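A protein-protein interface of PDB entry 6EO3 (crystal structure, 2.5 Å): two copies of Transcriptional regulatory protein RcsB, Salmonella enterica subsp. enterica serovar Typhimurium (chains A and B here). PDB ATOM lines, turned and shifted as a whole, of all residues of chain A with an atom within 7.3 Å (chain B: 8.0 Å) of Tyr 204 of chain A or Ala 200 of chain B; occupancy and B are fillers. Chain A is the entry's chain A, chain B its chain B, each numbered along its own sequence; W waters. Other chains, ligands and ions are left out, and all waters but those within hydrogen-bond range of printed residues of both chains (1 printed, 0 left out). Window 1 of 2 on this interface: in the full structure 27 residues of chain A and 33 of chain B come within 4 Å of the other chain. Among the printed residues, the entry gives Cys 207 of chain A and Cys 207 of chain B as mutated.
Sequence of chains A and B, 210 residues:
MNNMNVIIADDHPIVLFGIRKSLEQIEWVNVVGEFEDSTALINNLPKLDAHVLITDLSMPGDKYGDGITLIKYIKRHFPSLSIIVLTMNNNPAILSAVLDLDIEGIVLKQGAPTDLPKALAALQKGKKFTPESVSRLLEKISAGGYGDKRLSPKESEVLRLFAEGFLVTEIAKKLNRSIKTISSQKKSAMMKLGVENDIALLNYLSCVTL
N of Glu 196 of chain B sits at hydrogen-bond distance from O of Gly 194 of chain A (2.7 Å). OD1 of Asn 203 of chain A lies within hydrogen-bond range of OH of Tyr 204 of chain B, at 3.1 Å. The side-chain hydroxyl (OH) of Tyr 204 of chain A is in hydrogen-bond range of the side-chain amide oxygen (OD1) of Asn 203 of chain B. The side-chain hydroxyl (OG) of Ser 206 of chain A lies within hydrogen-bond range of the side-chain amide nitrogen (ND2) of Asn 91 of chain B. SG of Cys 207 of chain A is disulfide-bonded to SG of Cys 207 of chain B, at 2.0 Å. The backbone carbonyl oxygen of Val 195 of chain A sits close to the side-chain carboxylate of Glu 196 of chain B (3.4 Å). SG of Cys 207 of chain A lies close to O of Asn 203 of chain B, 3.4 Å away. The backbone carbonyl oxygen (O) of Tyr 204 of chain B sits close to the side-chain sulfur (SG) of Cys 207 of chain A, 3.5 Å away.
The backbone carbonyl oxygen (O) of Leu 202 of chain A sits at hydrogen-bond distance from the side-chain hydroxyl (OG) of Ser 206 of chain A, 3.5 Å away. The backbone carbonyl oxygen of Met 190 of chain B is in hydrogen-bond range of the backbone NH of Val 195 of chain B (3.0 Å). O of Leu 202 of chain B is in hydrogen-bond range of OG of Ser 206 of chain B, 3.3 Å away.
Among the printed residues, merely in contact across the chains: Asn 91 of chain A with Leu 202 of chain B (3.1 Å), Asn 203 of chain A with Pro 92 of chain B (3.3 Å), Leu 193 of chain A with Ala 200 of chain B (3.3 Å), Ala 200 of chain A with Leu 193 of chain B (3.3 Å), Leu 202 of chain A with Asn 90 of chain B (3.3 Å), Gly 194 of chain A with Asn 197 of chain B (3.3 Å), Ala 200 of chain A with Gly 194 of chain B (3.4 Å), Val 195 of chain A with Gly 194 of chain B (3.4 Å), Gly 194 of chain A with Val 195 of chain B (3.5 Å), Leu 202 of chain A with Pro 92 of chain B (3.5 Å), Asn 91 of chain A with Asp 198 of chain B (3.7 Å), Gly 194 of chain A with Ala 200 of chain B (3.7 Å), Ala 93 of chain A with Leu 202 of chain B (3.7 Å), Cys 207 of chain A with Ser 206 of chain B (3.7 Å), Asn 203 of chain A with Asn 91 of chain B (3.8 Å), Tyr 204 of chain A with Ala 200 of chain B (3.8 Å), Ile 199 of chain A with Pro 92 of chain B (3.8 Å) and Asn 91 of chain A with Ile 199 of chain B (3.9 Å).
Tyr 204 of chain A touches two residues of chain B. Of the printed residues of chain A, Cys 207 of chain B touches Cys 207 (2.0 Å). Printed residues of chain A within 4 Å of Pro 92 of chain B: Ile 199 (3.8 Å), Leu 202 (3.5 Å) and Asn 203 (3.3 Å). Of the printed residues of chain A, Ile 199 of chain B touches Asn 91 (3.9 Å). The nearest residue of chain B that does not touch Tyr 204 of chain A is Tyr 204 of chain B (4.4 Å). The nearest printed residue of chain A that does not touch Asn 91 of chain B is Leu 202 of chain A (4.7 Å).
Of the 19 printed residues of chain B, 16 touch a printed residue of chain A. Printed residues of chain A that touch a printed residue of chain B: Asn 91, Ala 93, Leu 193, Gly 194, Val 195, Ile 199, Ala 200, Leu 202, Asn 203, Tyr 204, Ser 206 and Cys 207. Hydrophobic or aromatic side chains of chain A that line the printed part of chain B: Ala 93, Val 195, Ala 200, Leu 202 and Tyr 204. Along chain A the printed residues that touch a printed residue of chain B span positions 91 to 207.
Asn 91 of chain A touches Leu 202 of chain B, but with the chains exchanged Leu 202 of chain A does not touch Asn 91 of chain B (4.7 Å). Cys 207 of chain B touches its own counterpart, Cys 207 of chain A. 14 positions are printed for both chains. Of the 26 pairs that touch across the chains among the printed residues, 9 have their exchanged pair printed and touching as well.
Water W1 bridges the side-chain carboxylate of Asp 198 of chain B (2.7 Å) and the side-chain amide nitrogen of Asn 91 of chain A (3.1 Å).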
ATOM      1  N   ASN A  91      20.636  26.687  -6.569  1.00  0.00           N
ATOM      2  CA  ASN A  91      21.310  25.821  -5.599  1.00  0.00           C
ATOM      3  C   ASN A  91      22.503  25.060  -6.196  1.00  0.00           C
ATOM      4  O   ASN A  91      22.340  24.306  -7.155  1.00  0.00           O
ATOM      5  CB  ASN A  91      20.338  24.816  -4.999  1.00  0.00           C
ATOM      6  CG  ASN A  91      20.911  24.125  -3.778  1.00  0.00           C
ATOM      7  OD1 ASN A  91      21.410  23.002  -3.859  1.00  0.00           O
ATOM      8  ND2 ASN A  91      20.866  24.810  -2.639  1.00  0.00           N
ATOM      9  N   ALA A  93      24.148  22.362  -5.409  1.00  0.00           N
ATOM     10  CA  ALA A  93      23.964  20.899  -5.516  1.00  0.00           C
ATOM     11  C   ALA A  93      23.085  20.483  -6.706  1.00  0.00           C
ATOM     12  O   ALA A  93      23.320  19.443  -7.323  1.00  0.00           O
ATOM     13  CB  ALA A  93      23.408  20.326  -4.226  1.00  0.00           C
ATOM     14  N   TYR A 146      30.570  20.697  -0.489  1.00  0.00           N
ATOM     15  CA  TYR A 146      29.733  20.704   0.715  1.00  0.00           C
ATOM     16  C   TYR A 146      29.613  22.056   1.474  1.00  0.00           C
ATOM     17  O   TYR A 146      28.909  22.121   2.482  1.00  0.00           O
ATOM     18  CB  TYR A 146      30.199  19.590   1.672  1.00  0.00           C
ATOM     19  CG  TYR A 146      31.698  19.562   1.929  1.00  0.00           C
ATOM     20  CD1 TYR A 146      32.327  20.598   2.623  1.00  0.00           C
ATOM     21  CD2 TYR A 146      32.484  18.493   1.492  1.00  0.00           C
ATOM     22  CE1 TYR A 146      33.691  20.577   2.861  1.00  0.00           C
ATOM     23  CE2 TYR A 146      33.851  18.464   1.729  1.00  0.00           C
ATOM     24  CZ  TYR A 146      34.448  19.509   2.413  1.00  0.00           C
ATOM     25  OH  TYR A 146      35.801  19.494   2.653  1.00  0.00           O
ATOM     26  N   GLY A 147      30.275  23.115   0.999  1.00  0.00           N
ATOM     27  CA  GLY A 147      30.222  24.435   1.651  1.00  0.00           C
ATOM     28  C   GLY A 147      31.452  25.305   1.417  1.00  0.00           C
ATOM     29  O   GLY A 147      32.549  24.796   1.172  1.00  0.00           O
ATOM     30  N   LEU A 159      36.384  13.258  11.558  1.00  0.00           N
ATOM     31  CA  LEU A 159      35.219  12.657  10.926  1.00  0.00           C
ATOM     32  C   LEU A 159      35.536  11.311  10.282  1.00  0.00           C
ATOM     33  O   LEU A 159      34.740  10.379  10.373  1.00  0.00           O
ATOM     34  CB  LEU A 159      34.625  13.604   9.892  1.00  0.00           C
ATOM     35  CG  LEU A 159      34.007  14.903  10.417  1.00  0.00           C
ATOM     36  CD1 LEU A 159      33.304  15.610   9.272  1.00  0.00           C
ATOM     37  CD2 LEU A 159      33.040  14.679  11.566  1.00  0.00           C
ATOM     38  N   LYS A 192      29.331  22.850   9.646  1.00  0.00           N
ATOM     39  CA  LYS A 192      29.764  23.156   8.279  1.00  0.00           C
ATOM     40  C   LYS A 192      29.066  22.302   7.218  1.00  0.00           C
ATOM     41  O   LYS A 192      28.721  22.802   6.144  1.00  0.00           O
ATOM     42  CB  LYS A 192      31.269  22.969   8.149  1.00  0.00           C
ATOM     43  CG  LYS A 192      32.095  23.970   8.932  1.00  0.00           C
ATOM     44  CD  LYS A 192      33.574  23.687   8.734  1.00  0.00           C
ATOM     45  CE  LYS A 192      34.452  24.766   9.332  1.00  0.00           C
ATOM     46  NZ  LYS A 192      35.874  24.535   8.966  1.00  0.00           N
ATOM     47  N   LEU A 193      28.874  21.018   7.512  1.00  0.00           N
ATOM     48  CA  LEU A 193      28.217  20.098   6.574  1.00  0.00           C
ATOM     49  C   LEU A 193      26.702  20.208   6.616  1.00  0.00           C
ATOM     50  O   LEU A 193      26.033  19.729   5.701  1.00  0.00           O
ATOM     51  CB  LEU A 193      28.611  18.645   6.861  1.00  0.00           C
ATOM     52  CG  LEU A 193      30.084  18.261   6.726  1.00  0.00           C
ATOM     53  CD1 LEU A 193      30.288  16.816   7.156  1.00  0.00           C
ATOM     54  CD2 LEU A 193      30.595  18.466   5.306  1.00  0.00           C
ATOM     55  N   GLY A 194      26.171  20.803   7.685  1.00  0.00           N
ATOM     56  CA  GLY A 194      24.724  21.011   7.849  1.00  0.00           C
ATOM     57  C   GLY A 194      23.941  19.799   8.328  1.00  0.00           C
ATOM     58  O   GLY A 194      22.799  19.586   7.921  1.00  0.00           O
ATOM     59  N   VAL A 195      24.551  19.008   9.202  1.00  0.00           N
ATOM     60  CA  VAL A 195      23.907  17.825   9.771  1.00  0.00           C
ATOM     61  C   VAL A 195      23.772  17.968  11.292  1.00  0.00           C
ATOM     62  O   VAL A 195      24.676  18.450  11.961  1.00  0.00           O
ATOM     63  CB  VAL A 195      24.662  16.537   9.394  1.00  0.00           C
ATOM     64  CG1 VAL A 195      24.634  16.355   7.883  1.00  0.00           C
ATOM     65  CG2 VAL A 195      26.104  16.537   9.919  1.00  0.00           C
ATOM     66  N   ASP A 198      24.281  12.295  14.658  1.00  0.00           N
ATOM     67  CA  ASP A 198      25.246  11.289  14.209  1.00  0.00           C
ATOM     68  C   ASP A 198      24.699  10.370  13.115  1.00  0.00           C
ATOM     69  O   ASP A 198      25.425   9.971  12.198  1.00  0.00           O
ATOM     70  CB  ASP A 198      25.716  10.458  15.403  1.00  0.00           C
ATOM     71  CG  ASP A 198      26.571  11.258  16.370  1.00  0.00           C
ATOM     72  OD1 ASP A 198      26.845  12.456  16.116  1.00  0.00           O
ATOM     73  OD2 ASP A 198      26.984  10.681  17.394  1.00  0.00           O
ATOM     74  N   ILE A 199      23.421  10.034  13.214  1.00  0.00           N
ATOM     75  CA  ILE A 199      22.788   9.226  12.186  1.00  0.00           C
ATOM     76  C   ILE A 199      22.828   9.953  10.843  1.00  0.00           C
ATOM     77  O   ILE A 199      23.144   9.356   9.815  1.00  0.00           O
ATOM     78  CB  ILE A 199      21.347   8.848  12.571  1.00  0.00           C
ATOM     79  CG1 ILE A 199      21.380   7.866  13.749  1.00  0.00           C
ATOM     80  CG2 ILE A 199      20.614   8.220  11.391  1.00  0.00           C
ATOM     81  CD1 ILE A 199      20.029   7.607  14.387  1.00  0.00           C
ATOM     82  N   ALA A 200      22.511  11.238  10.860  1.00  0.00           N
ATOM     83  CA  ALA A 200      22.540  12.049   9.657  1.00  0.00           C
ATOM     84  C   ALA A 200      23.978  12.221   9.204  1.00  0.00           C
ATOM     85  O   ALA A 200      24.277  12.130   8.010  1.00  0.00           O
ATOM     86  CB  ALA A 200      21.901  13.403   9.914  1.00  0.00           C
ATOM     87  N   LEU A 201      24.866  12.462  10.164  1.00  0.00           N
ATOM     88  CA  LEU A 201      26.294  12.612   9.878  1.00  0.00           C
ATOM     89  C   LEU A 201      26.867  11.403   9.130  1.00  0.00           C
ATOM     90  O   LEU A 201      27.513  11.548   8.086  1.00  0.00           O
ATOM     91  CB  LEU A 201      27.064  12.808  11.183  1.00  0.00           C
ATOM     92  CG  LEU A 201      28.588  12.928  11.087  1.00  0.00           C
ATOM     93  CD1 LEU A 201      28.999  14.073  10.173  1.00  0.00           C
ATOM     94  CD2 LEU A 201      29.179  13.113  12.477  1.00  0.00           C
ATOM     95  N   LEU A 202      26.615  10.215   9.673  1.00  0.00           N
ATOM     96  CA  LEU A 202      27.193   8.974   9.153  1.00  0.00           C
ATOM     97  C   LEU A 202      26.564   8.520   7.835  1.00  0.00           C
ATOM     98  O   LEU A 202      27.232   7.905   7.009  1.00  0.00           O
ATOM     99  CB  LEU A 202      27.088   7.869  10.212  1.00  0.00           C
ATOM    100  CG  LEU A 202      27.968   8.084  11.449  1.00  0.00           C
ATOM    101  CD1 LEU A 202      27.523   7.202  12.596  1.00  0.00           C
ATOM    102  CD2 LEU A 202      29.426   7.817  11.131  1.00  0.00           C
ATOM    103  N   ASN A 203      25.285   8.815   7.645  1.00  0.00           N
ATOM    104  CA  ASN A 203      24.641   8.591   6.350  1.00  0.00           C
ATOM    105  C   ASN A 203      25.245   9.493   5.280  1.00  0.00           C
ATOM    106  O   ASN A 203      25.557   9.042   4.181  1.00  0.00           O
ATOM    107  CB  ASN A 203      23.127   8.825   6.435  1.00  0.00           C
ATOM    108  CG  ASN A 203      22.387   7.728   7.198  1.00  0.00           C
ATOM    109  OD1 ASN A 203      21.295   7.958   7.725  1.00  0.00           O
ATOM    110  ND2 ASN A 203      22.955   6.532   7.246  1.00  0.00           N
ATOM    111  N   TYR A 204      25.413  10.766   5.617  1.00  0.00           N
ATOM    112  CA  TYR A 204      26.032  11.751   4.724  1.00  0.00           C
ATOM    113  C   TYR A 204      27.430  11.336   4.249  1.00  0.00           C
ATOM    114  O   TYR A 204      27.773  11.515   3.079  1.00  0.00           O
ATOM    115  CB  TYR A 204      26.118  13.089   5.457  1.00  0.00           C
ATOM    116  CG  TYR A 204      26.494  14.288   4.614  1.00  0.00           C
ATOM    117  CD1 TYR A 204      25.526  14.978   3.886  1.00  0.00           C
ATOM    118  CD2 TYR A 204      27.807  14.766   4.581  1.00  0.00           C
ATOM    119  CE1 TYR A 204      25.854  16.091   3.127  1.00  0.00           C
ATOM    120  CE2 TYR A 204      28.144  15.883   3.826  1.00  0.00           C
ATOM    121  CZ  TYR A 204      27.163  16.544   3.098  1.00  0.00           C
ATOM    122  OH  TYR A 204      27.472  17.662   2.342  1.00  0.00           O
ATOM    123  N   LEU A 205      28.224  10.787   5.166  1.00  0.00           N
ATOM    124  CA  LEU A 205      29.604  10.365   4.877  1.00  0.00           C
ATOM    125  C   LEU A 205      29.728   9.167   3.922  1.00  0.00           C
ATOM    126  O   LEU A 205      30.733   9.045   3.215  1.00  0.00           O
ATOM    127  CB  LEU A 205      30.353  10.058   6.182  1.00  0.00           C
ATOM    128  CG  LEU A 205      31.070  11.206   6.911  1.00  0.00           C
ATOM    129  CD1 LEU A 205      30.474  12.579   6.642  1.00  0.00           C
ATOM    130  CD2 LEU A 205      31.094  10.942   8.408  1.00  0.00           C
ATOM    131  N   SER A 206      28.728   8.287   3.905  1.00  0.00           N
ATOM    132  CA  SER A 206      28.725   7.138   2.986  1.00  0.00           C
ATOM    133  C   SER A 206      28.447   7.586   1.551  1.00  0.00           C
ATOM    134  O   SER A 206      29.138   7.168   0.623  1.00  0.00           O
ATOM    135  CB  SER A 206      27.700   6.094   3.430  1.00  0.00           C
ATOM    136  OG  SER A 206      28.101   5.495   4.652  1.00  0.00           O
ATOM    137  N   CYS A 207      27.425   8.427   1.385  1.00  0.00           N
ATOM    138  CA  CYS A 207      27.195   9.157   0.129  1.00  0.00           C
ATOM    139  C   CYS A 207      28.513   9.796  -0.333  1.00  0.00           C
ATOM    140  O   CYS A 207      29.122   9.353  -1.309  1.00  0.00           O
ATOM    141  CB  CYS A 207      26.133  10.261   0.312  1.00  0.00           C
ATOM    142  SG  CYS A 207      24.391   9.893  -0.039  1.00  0.00           S
ATOM    143  N   VAL A 208      28.946  10.828   0.392  1.00  0.00           N
ATOM    144  CA  VAL A 208      30.196  11.531   0.100  1.00  0.00           C
ATOM    145  C   VAL A 208      31.384  10.727   0.622  1.00  0.00           C
ATOM    146  O   VAL A 208      32.372  11.293   1.085  1.00  0.00           O
ATOM    147  CB  VAL A 208      30.178  12.919   0.722  1.00  0.00           C
ATOM    148  N   ASN B  90      30.602   3.097   9.586  1.00  0.00           N
ATOM    149  CA  ASN B  90      29.411   3.029  10.403  1.00  0.00           C
ATOM    150  C   ASN B  90      28.345   3.691   9.541  1.00  0.00           C
ATOM    151  O   ASN B  90      28.356   4.913   9.367  1.00  0.00           O
ATOM    152  CB  ASN B  90      29.645   3.791  11.715  1.00  0.00           C
ATOM    153  CG  ASN B  90      28.986   3.140  12.915  1.00  0.00           C
ATOM    154  OD1 ASN B  90      28.198   2.209  12.785  1.00  0.00           O
ATOM    155  ND2 ASN B  90      29.313   3.639  14.101  1.00  0.00           N
ATOM    156  N   ASN B  91      27.479   2.881   8.942  1.00  0.00           N
ATOM    157  CA  ASN B  91      26.561   3.357   7.915  1.00  0.00           C
ATOM    158  C   ASN B  91      25.127   3.003   8.290  1.00  0.00           C
ATOM    159  O   ASN B  91      24.598   1.992   7.835  1.00  0.00           O
ATOM    160  CB  ASN B  91      26.948   2.752   6.561  1.00  0.00           C
ATOM    161  CG  ASN B  91      26.061   3.224   5.419  1.00  0.00           C
ATOM    162  OD1 ASN B  91      25.026   3.847   5.624  1.00  0.00           O
ATOM    163  ND2 ASN B  91      26.474   2.923   4.202  1.00  0.00           N
ATOM    164  N   PRO B  92      24.482   3.853   9.108  1.00  0.00           N
ATOM    165  CA  PRO B  92      23.198   3.506   9.727  1.00  0.00           C
ATOM    166  C   PRO B  92      22.183   2.875   8.775  1.00  0.00           C
ATOM    167  O   PRO B  92      21.501   1.926   9.153  1.00  0.00           O
ATOM    168  CB  PRO B  92      22.682   4.842  10.260  1.00  0.00           C
ATOM    169  CG  PRO B  92      23.900   5.678  10.447  1.00  0.00           C
ATOM    170  CD  PRO B  92      24.942   5.199   9.485  1.00  0.00           C
ATOM    171  N   MET B 190      13.096  17.567   6.371  1.00  0.00           N
ATOM    172  CA  MET B 190      14.525  17.839   6.643  1.00  0.00           C
ATOM    173  C   MET B 190      14.870  17.553   8.109  1.00  0.00           C
ATOM    174  O   MET B 190      15.939  17.025   8.422  1.00  0.00           O
ATOM    175  CB  MET B 190      14.907  19.302   6.310  1.00  0.00           C
ATOM    176  CG  MET B 190      14.634  19.752   4.883  1.00  0.00           C
ATOM    177  SD  MET B 190      15.402  21.317   4.402  1.00  0.00           S
ATOM    178  CE  MET B 190      14.798  22.489   5.589  1.00  0.00           C
ATOM    179  N   LEU B 193      15.184  13.822   8.853  1.00  0.00           N
ATOM    180  CA  LEU B 193      16.441  13.268   8.322  1.00  0.00           C
ATOM    181  C   LEU B 193      17.691  13.821   9.007  1.00  0.00           C
ATOM    182  O   LEU B 193      18.795  13.311   8.788  1.00  0.00           O
ATOM    183  CB  LEU B 193      16.546  13.547   6.818  1.00  0.00           C
ATOM    184  CG  LEU B 193      15.401  13.020   5.962  1.00  0.00           C
ATOM    185  CD1 LEU B 193      15.606  13.455   4.518  1.00  0.00           C
ATOM    186  CD2 LEU B 193      15.305  11.508   6.059  1.00  0.00           C
ATOM    187  N   GLY B 194      17.523  14.877   9.796  1.00  0.00           N
ATOM    188  CA  GLY B 194      18.644  15.518  10.498  1.00  0.00           C
ATOM    189  C   GLY B 194      19.530  16.425   9.643  1.00  0.00           C
ATOM    190  O   GLY B 194      20.718  16.561   9.932  1.00  0.00           O
ATOM    191  N   VAL B 195      18.965  17.055   8.610  1.00  0.00           N
ATOM    192  CA  VAL B 195      19.749  17.934   7.721  1.00  0.00           C
ATOM    193  C   VAL B 195      19.268  19.390   7.827  1.00  0.00           C
ATOM    194  O   VAL B 195      18.072  19.655   7.825  1.00  0.00           O
ATOM    195  CB  VAL B 195      19.764  17.454   6.233  1.00  0.00           C
ATOM    196  CG1 VAL B 195      20.232  16.013   6.136  1.00  0.00           C
ATOM    197  CG2 VAL B 195      18.407  17.597   5.566  1.00  0.00           C
ATOM    198  N   GLU B 196      20.218  20.315   7.912  1.00  0.00           N
ATOM    199  CA  GLU B 196      19.944  21.724   8.219  1.00  0.00           C
ATOM    200  C   GLU B 196      19.714  22.578   6.966  1.00  0.00           C
ATOM    201  O   GLU B 196      18.957  23.539   7.006  1.00  0.00           O
ATOM    202  CB  GLU B 196      21.103  22.342   9.033  1.00  0.00           C
ATOM    203  CG  GLU B 196      21.538  21.571  10.282  1.00  0.00           C
ATOM    204  CD  GLU B 196      22.762  22.181  10.986  1.00  0.00           C
ATOM    205  OE1 GLU B 196      23.176  23.312  10.627  1.00  0.00           O
ATOM    206  OE2 GLU B 196      23.317  21.533  11.909  1.00  0.00           O
ATOM    207  N   ASN B 197      20.381  22.241   5.864  1.00  0.00           N
ATOM    208  CA  ASN B 197      20.320  23.064   4.657  1.00  0.00           C
ATOM    209  C   ASN B 197      20.104  22.239   3.389  1.00  0.00           C
ATOM    210  O   ASN B 197      20.186  21.008   3.411  1.00  0.00           O
ATOM    211  CB  ASN B 197      21.562  23.977   4.548  1.00  0.00           C
ATOM    212  CG  ASN B 197      22.872  23.203   4.460  1.00  0.00           C
ATOM    213  OD1 ASN B 197      23.225  22.677   3.405  1.00  0.00           O
ATOM    214  ND2 ASN B 197      23.616  23.165   5.556  1.00  0.00           N
ATOM    215  N   ASP B 198      19.812  22.943   2.296  1.00  0.00           N
ATOM    216  CA  ASP B 198      19.372  22.336   1.037  1.00  0.00           C
ATOM    217  C   ASP B 198      20.477  21.577   0.331  1.00  0.00           C
ATOM    218  O   ASP B 198      20.226  20.532  -0.274  1.00  0.00           O
ATOM    219  CB  ASP B 198      18.812  23.412   0.098  1.00  0.00           C
ATOM    220  CG  ASP B 198      17.476  23.968   0.569  1.00  0.00           C
ATOM    221  OD1 ASP B 198      16.800  23.315   1.390  1.00  0.00           O
ATOM    222  OD2 ASP B 198      17.087  25.061   0.108  1.00  0.00           O
ATOM    223  N   ILE B 199      21.690  22.123   0.392  1.00  0.00           N
ATOM    224  CA  ILE B 199      22.886  21.440  -0.105  1.00  0.00           C
ATOM    225  C   ILE B 199      23.056  20.098   0.607  1.00  0.00           C
ATOM    226  O   ILE B 199      23.270  19.073  -0.028  1.00  0.00           O
ATOM    227  CB  ILE B 199      24.142  22.315   0.082  1.00  0.00           C
ATOM    228  CG1 ILE B 199      24.081  23.513  -0.875  1.00  0.00           C
ATOM    229  CG2 ILE B 199      25.415  21.500  -0.148  1.00  0.00           C
ATOM    230  CD1 ILE B 199      25.094  24.607  -0.602  1.00  0.00           C
ATOM    231  N   ALA B 200      22.961  20.127   1.932  1.00  0.00           N
ATOM    232  CA  ALA B 200      23.101  18.935   2.759  1.00  0.00           C
ATOM    233  C   ALA B 200      21.968  17.966   2.478  1.00  0.00           C
ATOM    234  O   ALA B 200      22.172  16.755   2.431  1.00  0.00           O
ATOM    235  CB  ALA B 200      23.108  19.315   4.236  1.00  0.00           C
ATOM    236  N   LEU B 201      20.770  18.511   2.309  1.00  0.00           N
ATOM    237  CA  LEU B 201      19.608  17.714   1.919  1.00  0.00           C
ATOM    238  C   LEU B 201      19.824  16.960   0.606  1.00  0.00           C
ATOM    239  O   LEU B 201      19.570  15.762   0.538  1.00  0.00           O
ATOM    240  CB  LEU B 201      18.371  18.604   1.805  1.00  0.00           C
ATOM    241  CG  LEU B 201      17.077  17.936   1.329  1.00  0.00           C
ATOM    242  CD1 LEU B 201      16.595  16.906   2.338  1.00  0.00           C
ATOM    243  CD2 LEU B 201      16.011  18.991   1.082  1.00  0.00           C
ATOM    244  N   LEU B 202      20.298  17.660  -0.423  1.00  0.00           N
ATOM    245  CA  LEU B 202      20.437  17.067  -1.762  1.00  0.00           C
ATOM    246  C   LEU B 202      21.566  16.054  -1.838  1.00  0.00           C
ATOM    247  O   LEU B 202      21.420  14.993  -2.459  1.00  0.00           O
ATOM    248  CB  LEU B 202      20.645  18.151  -2.812  1.00  0.00           C
ATOM    249  CG  LEU B 202      19.384  18.989  -3.060  1.00  0.00           C
ATOM    250  CD1 LEU B 202      19.728  20.349  -3.646  1.00  0.00           C
ATOM    251  CD2 LEU B 202      18.422  18.255  -3.973  1.00  0.00           C
ATOM    252  N   ASN B 203      22.697  16.378  -1.221  1.00  0.00           N
ATOM    253  CA  ASN B 203      23.774  15.406  -1.078  1.00  0.00           C
ATOM    254  C   ASN B 203      23.239  14.182  -0.363  1.00  0.00           C
ATOM    255  O   ASN B 203      23.442  13.063  -0.834  1.00  0.00           O
ATOM    256  CB  ASN B 203      24.958  15.976  -0.300  1.00  0.00           C
ATOM    257  CG  ASN B 203      25.663  17.112  -1.026  1.00  0.00           C
ATOM    258  OD1 ASN B 203      26.092  18.080  -0.393  1.00  0.00           O
ATOM    259  ND2 ASN B 203      25.795  17.006  -2.348  1.00  0.00           N
ATOM    260  N   TYR B 204      22.531  14.413   0.751  1.00  0.00           N
ATOM    261  CA  TYR B 204      21.916  13.338   1.547  1.00  0.00           C
ATOM    262  C   TYR B 204      21.075  12.402   0.689  1.00  0.00           C
ATOM    263  O   TYR B 204      21.252  11.192   0.727  1.00  0.00           O
ATOM    264  CB  TYR B 204      21.037  13.906   2.681  1.00  0.00           C
ATOM    265  CG  TYR B 204      20.573  12.853   3.671  1.00  0.00           C
ATOM    266  CD1 TYR B 204      19.499  12.018   3.377  1.00  0.00           C
ATOM    267  CD2 TYR B 204      21.225  12.674   4.894  1.00  0.00           C
ATOM    268  CE1 TYR B 204      19.082  11.043   4.268  1.00  0.00           C
ATOM    269  CE2 TYR B 204      20.813  11.696   5.793  1.00  0.00           C
ATOM    270  CZ  TYR B 204      19.745  10.882   5.466  1.00  0.00           C
ATOM    271  OH  TYR B 204      19.319   9.912   6.335  1.00  0.00           O
ATOM    272  N   LEU B 205      20.153  12.977  -0.075  1.00  0.00           N
ATOM    273  CA  LEU B 205      19.222  12.193  -0.888  1.00  0.00           C
ATOM    274  C   LEU B 205      19.878  11.354  -1.995  1.00  0.00           C
ATOM    275  O   LEU B 205      19.272  10.384  -2.458  1.00  0.00           O
ATOM    276  CB  LEU B 205      18.124  13.094  -1.465  1.00  0.00           C
ATOM    277  CG  LEU B 205      17.205  13.719  -0.401  1.00  0.00           C
ATOM    278  CD1 LEU B 205      16.348  14.817  -1.009  1.00  0.00           C
ATOM    279  CD2 LEU B 205      16.336  12.674   0.299  1.00  0.00           C
ATOM    280  N   SER B 206      21.104  11.701  -2.394  1.00  0.00           N
ATOM    281  CA  SER B 206      21.904  10.838  -3.285  1.00  0.00           C
ATOM    282  C   SER B 206      21.938   9.381  -2.799  1.00  0.00           C
ATOM    283  O   SER B 206      22.098   8.469  -3.599  1.00  0.00           O
ATOM    284  CB  SER B 206      23.338  11.363  -3.431  1.00  0.00           C
ATOM    285  OG  SER B 206      23.350  12.734  -3.791  1.00  0.00           O
ATOM    286  N   CYS B 207      21.808   9.181  -1.487  1.00  0.00           N
ATOM    287  CA  CYS B 207      21.520   7.862  -0.907  1.00  0.00           C
ATOM    288  C   CYS B 207      20.069   7.814  -0.412  1.00  0.00           C
ATOM    289  O   CYS B 207      19.321   6.867  -0.640  1.00  0.00           O
ATOM    290  CB  CYS B 207      22.467   7.574   0.251  1.00  0.00           C
ATOM    291  SG  CYS B 207      24.209   7.866  -0.133  1.00  0.00           S
HETATM  292  O   HOH W   1      18.013  25.958  -2.223  1.00  0.00           O
